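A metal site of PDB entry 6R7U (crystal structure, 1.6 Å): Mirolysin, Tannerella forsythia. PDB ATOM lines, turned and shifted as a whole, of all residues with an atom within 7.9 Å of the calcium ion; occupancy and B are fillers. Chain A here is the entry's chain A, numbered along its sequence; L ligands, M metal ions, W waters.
Of the 16 residues printed, 3 come within 4 Å of the calcium ion.
The calcium ion is bound by OD1 of Asp 230, water W1, O of Ile 232, O of Thr 235, O2 of the ligand, OG1 of Thr 235, O1 of the ligand and O3 of the ligand. The calcium ion has eight donor atoms within binding distance.
Water W1 lies within hydrogen-bond range of O of Ile 218 (2.8 Å) and O of Pro 236 (2.9 Å).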
ATOM      1  N   HIS A 217      14.076  -4.456   6.788  1.00  0.00           N
ATOM      2  CA  HIS A 217      15.109  -3.850   7.621  1.00  0.00           C
ATOM      3  C   HIS A 217      14.454  -2.843   8.514  1.00  0.00           C
ATOM      4  O   HIS A 217      13.660  -2.026   8.045  1.00  0.00           O
ATOM      5  CB  HIS A 217      16.102  -3.159   6.711  1.00  0.00           C
ATOM      6  CG  HIS A 217      16.938  -4.198   6.043  1.00  0.00           C
ATOM      7  ND1 HIS A 217      17.509  -3.967   4.805  1.00  0.00           N
ATOM      8  CD2 HIS A 217      17.237  -5.456   6.441  1.00  0.00           C
ATOM      9  CE1 HIS A 217      18.185  -5.090   4.521  1.00  0.00           C
ATOM     10  NE2 HIS A 217      18.058  -6.003   5.488  1.00  0.00           N
ATOM     11  N   ILE A 218      14.836  -2.837   9.772  1.00  0.00           N
ATOM     12  CA  ILE A 218      14.196  -1.975  10.778  1.00  0.00           C
ATOM     13  C   ILE A 218      14.308  -0.464  10.458  1.00  0.00           C
ATOM     14  O   ILE A 218      13.390   0.322  10.832  1.00  0.00           O
ATOM     15  CB  ILE A 218      14.755  -2.320  12.178  1.00  0.00           C
ATOM     16  CG1 ILE A 218      14.034  -1.594  13.258  1.00  0.00           C
ATOM     17  CG2 ILE A 218      16.251  -2.020  12.258  1.00  0.00           C
ATOM     18  CD1 ILE A 218      14.299  -2.208  14.688  1.00  0.00           C
ATOM     19  N   TRP A 219      15.373  -0.071   9.734  1.00  0.00           N
ATOM     20  CA  TRP A 219      15.524   1.375   9.471  1.00  0.00           C
ATOM     21  C   TRP A 219      14.753   1.860   8.220  1.00  0.00           C
ATOM     22  O   TRP A 219      14.812   3.045   7.868  1.00  0.00           O
ATOM     23  CB  TRP A 219      16.972   1.733   9.328  1.00  0.00           C
ATOM     24  CG  TRP A 219      17.570   1.143   8.102  1.00  0.00           C
ATOM     25  CD1 TRP A 219      17.854   1.786   6.929  1.00  0.00           C
ATOM     26  CD2 TRP A 219      18.174  -0.137   8.023  1.00  0.00           C
ATOM     27  NE1 TRP A 219      18.497   0.919   6.070  1.00  0.00           N
ATOM     28  CE2 TRP A 219      18.694  -0.279   6.711  1.00  0.00           C
ATOM     29  CE3 TRP A 219      18.387  -1.166   8.954  1.00  0.00           C
ATOM     30  CZ2 TRP A 219      19.393  -1.425   6.309  1.00  0.00           C
ATOM     31  CZ3 TRP A 219      19.018  -2.332   8.525  1.00  0.00           C
ATOM     32  CH2 TRP A 219      19.532  -2.451   7.239  1.00  0.00           C
ATOM     33  N   GLY A 220      14.109   0.933   7.509  1.00  0.00           N
ATOM     34  CA  GLY A 220      13.260   1.341   6.409  1.00  0.00           C
ATOM     35  C   GLY A 220      13.896   1.449   5.033  1.00  0.00           C
ATOM     36  O   GLY A 220      13.229   1.861   4.085  1.00  0.00           O
ATOM     37  N   GLY A 228      11.308   6.278   5.381  1.00  0.00           N
ATOM     38  CA  GLY A 228      11.015   4.881   5.107  1.00  0.00           C
ATOM     39  C   GLY A 228      10.460   4.192   6.352  1.00  0.00           C
ATOM     40  O   GLY A 228      10.518   4.737   7.459  1.00  0.00           O
ATOM     41  N   THR A 229       9.909   2.993   6.191  1.00  0.00           N
ATOM     42  CA  THR A 229       9.294   2.305   7.320  1.00  0.00           C
ATOM     43  C   THR A 229       9.512   0.795   7.172  1.00  0.00           C
ATOM     44  O   THR A 229       9.664   0.273   6.050  1.00  0.00           O
ATOM     45  CB  THR A 229       7.769   2.618   7.337  1.00  0.00           C
ATOM     46  OG1 THR A 229       7.177   1.984   8.496  1.00  0.00           O
ATOM     47  CG2 THR A 229       7.064   2.125   6.057  1.00  0.00           C
ATOM     48  N   ASP A 230       9.437   0.089   8.291  1.00  0.00           N
ATOM     49  CA  ASP A 230       9.478  -1.352   8.238  1.00  0.00           C
ATOM     50  C   ASP A 230       8.034  -1.861   8.463  1.00  0.00           C
ATOM     51  O   ASP A 230       7.813  -3.064   8.573  1.00  0.00           O
ATOM     52  CB  ASP A 230      10.515  -1.930   9.240  1.00  0.00           C
ATOM     53  CG  ASP A 230      10.124  -1.801  10.721  1.00  0.00           C
ATOM     54  OD1 ASP A 230       9.264  -0.939  11.052  1.00  0.00           O
ATOM     55  OD2 ASP A 230      10.666  -2.569  11.545  1.00  0.00           O
ATOM     56  N   ASN A 231       7.048  -0.921   8.540  1.00  0.00           N
ATOM     57  CA  ASN A 231       5.635  -1.266   8.717  1.00  0.00           C
ATOM     58  C   ASN A 231       5.336  -1.968  10.045  1.00  0.00           C
ATOM     59  O   ASN A 231       4.250  -2.548  10.198  1.00  0.00           O
ATOM     60  CB  ASN A 231       5.143  -2.123   7.562  1.00  0.00           C
ATOM     61  CG  ASN A 231       5.199  -1.409   6.240  1.00  0.00           C
ATOM     62  OD1 ASN A 231       5.708  -1.942   5.259  1.00  0.00           O
ATOM     63  ND2 ASN A 231       4.654  -0.196   6.181  1.00  0.00           N
ATOM     64  N   ILE A 232       6.223  -1.851  11.030  1.00  0.00           N
ATOM     65  CA  ILE A 232       6.027  -2.417  12.365  1.00  0.00           C
ATOM     66  C   ILE A 232       6.001  -1.246  13.355  1.00  0.00           C
ATOM     67  O   ILE A 232       7.028  -0.594  13.515  1.00  0.00           O
ATOM     68  CB  ILE A 232       7.092  -3.477  12.738  1.00  0.00           C
ATOM     69  CG1 ILE A 232       7.193  -4.604  11.640  1.00  0.00           C
ATOM     70  CG2 ILE A 232       6.815  -4.039  14.153  1.00  0.00           C
ATOM     71  CD1 ILE A 232       5.984  -5.455  11.489  1.00  0.00           C
ATOM     72  N   ALA A 233       4.879  -1.014  14.023  1.00  0.00           N
ATOM     73  CA  ALA A 233       4.829   0.106  14.954  1.00  0.00           C
ATOM     74  C   ALA A 233       5.761  -0.093  16.158  1.00  0.00           C
ATOM     75  O   ALA A 233       6.335   0.875  16.614  1.00  0.00           O
ATOM     76  CB  ALA A 233       3.411   0.327  15.470  1.00  0.00           C
ATOM     77  N   ASP A 234       5.966  -1.336  16.645  1.00  0.00           N
ATOM     78  CA  ASP A 234       6.735  -1.455  17.881  1.00  0.00           C
ATOM     79  C   ASP A 234       8.239  -1.509  17.671  1.00  0.00           C
ATOM     80  O   ASP A 234       8.970  -1.676  18.641  1.00  0.00           O
ATOM     81  CB  ASP A 234       6.250  -2.601  18.754  1.00  0.00           C
ATOM     82  CG  ASP A 234       6.410  -3.976  18.188  1.00  0.00           C
ATOM     83  OD1 ASP A 234       6.971  -4.098  17.091  1.00  0.00           O
ATOM     84  OD2 ASP A 234       5.931  -4.960  18.862  1.00  0.00           O
ATOM     85  N   THR A 235       8.720  -1.338  16.429  1.00  0.00           N
ATOM     86  CA  THR A 235      10.125  -1.128  16.179  1.00  0.00           C
ATOM     87  C   THR A 235      10.279   0.397  16.016  1.00  0.00           C
ATOM     88  O   THR A 235       9.667   0.979  15.142  1.00  0.00           O
ATOM     89  CB  THR A 235      10.640  -1.844  14.936  1.00  0.00           C
ATOM     90  OG1 THR A 235       9.798  -1.514  13.843  1.00  0.00           O
ATOM     91  CG2 THR A 235      10.673  -3.357  15.110  1.00  0.00           C
ATOM     92  N   PRO A 236      11.043   1.057  16.895  1.00  0.00           N
ATOM     93  CA  PRO A 236      11.179   2.516  16.776  1.00  0.00           C
ATOM     94  C   PRO A 236      11.618   2.962  15.401  1.00  0.00           C
ATOM     95  O   PRO A 236      12.545   2.316  14.819  1.00  0.00           O
ATOM     96  CB  PRO A 236      12.276   2.851  17.792  1.00  0.00           C
ATOM     97  CG  PRO A 236      12.196   1.724  18.834  1.00  0.00           C
ATOM     98  CD  PRO A 236      11.860   0.501  17.995  1.00  0.00           C
ATOM     99  N   ASN A 237      11.104   4.127  14.975  1.00  0.00           N
ATOM    100  CA  ASN A 237      11.556   4.742  13.702  1.00  0.00           C
ATOM    101  C   ASN A 237      13.049   4.950  13.818  1.00  0.00           C
ATOM    102  O   ASN A 237      13.541   5.293  14.899  1.00  0.00           O
ATOM    103  CB  ASN A 237      10.840   6.017  13.411  1.00  0.00           C
ATOM    104  CG  ASN A 237      11.107   6.536  12.021  1.00  0.00           C
ATOM    105  OD1 ASN A 237      11.699   5.857  11.187  1.00  0.00           O
ATOM    106  ND2 ASN A 237      10.635   7.748  11.727  1.00  0.00           N
ATOM    107  N   GLN A 238      13.783   4.578  12.785  1.00  0.00           N
ATOM    108  CA  GLN A 238      15.229   4.610  12.824  1.00  0.00           C
ATOM    109  C   GLN A 238      15.767   5.218  11.553  1.00  0.00           C
ATOM    110  O   GLN A 238      15.205   4.954  10.484  1.00  0.00           O
ATOM    111  CB  GLN A 238      15.731   3.191  12.973  1.00  0.00           C
ATOM    112  CG  GLN A 238      17.237   2.973  13.116  1.00  0.00           C
ATOM    113  CD  GLN A 238      17.543   1.518  13.389  1.00  0.00           C
ATOM    114  OE1 GLN A 238      16.898   0.916  14.237  1.00  0.00           O
ATOM    115  NE2 GLN A 238      18.544   0.926  12.727  1.00  0.00           N
ATOM    116  N   GLN A 282       6.577  -7.789  15.003  1.00  0.00           N
ATOM    117  CA  GLN A 282       7.225  -8.553  13.938  1.00  0.00           C
ATOM    118  C   GLN A 282       6.675  -9.977  13.935  1.00  0.00           C
ATOM    119  O   GLN A 282       6.375 -10.555  12.879  1.00  0.00           O
ATOM    120  CB  GLN A 282       8.725  -8.555  14.199  1.00  0.00           C
ATOM    121  CG  GLN A 282       9.382  -7.311  13.676  1.00  0.00           C
ATOM    122  CD  GLN A 282      10.840  -7.216  14.105  1.00  0.00           C
ATOM    123  OE1 GLN A 282      11.222  -7.656  15.190  1.00  0.00           O
ATOM    124  NE2 GLN A 282      11.666  -6.595  13.273  1.00  0.00           N
HETATM  125  C1  LIG L   1       6.801   2.548  11.771  1.00  0.00           C
HETATM  126  O1  LIG L   1       7.104   1.207  11.373  1.00  0.00           O
HETATM  127  C2  LIG L   1       8.008   3.408  12.069  1.00  0.00           C
HETATM  128  O2  LIG L   1       8.654   2.983  13.277  1.00  0.00           O
HETATM  129  C3  LIG L   1       8.987   3.363  10.917  1.00  0.00           C
HETATM  130  O3  LIG L   1       9.705   2.125  10.883  1.00  0.00           O
HETATM  131 CA    CA M   1       9.046   0.598  12.793  1.00  0.00          CA
HETATM  132  O   HOH W   1      11.374   0.760  12.713  1.00  0.00           O
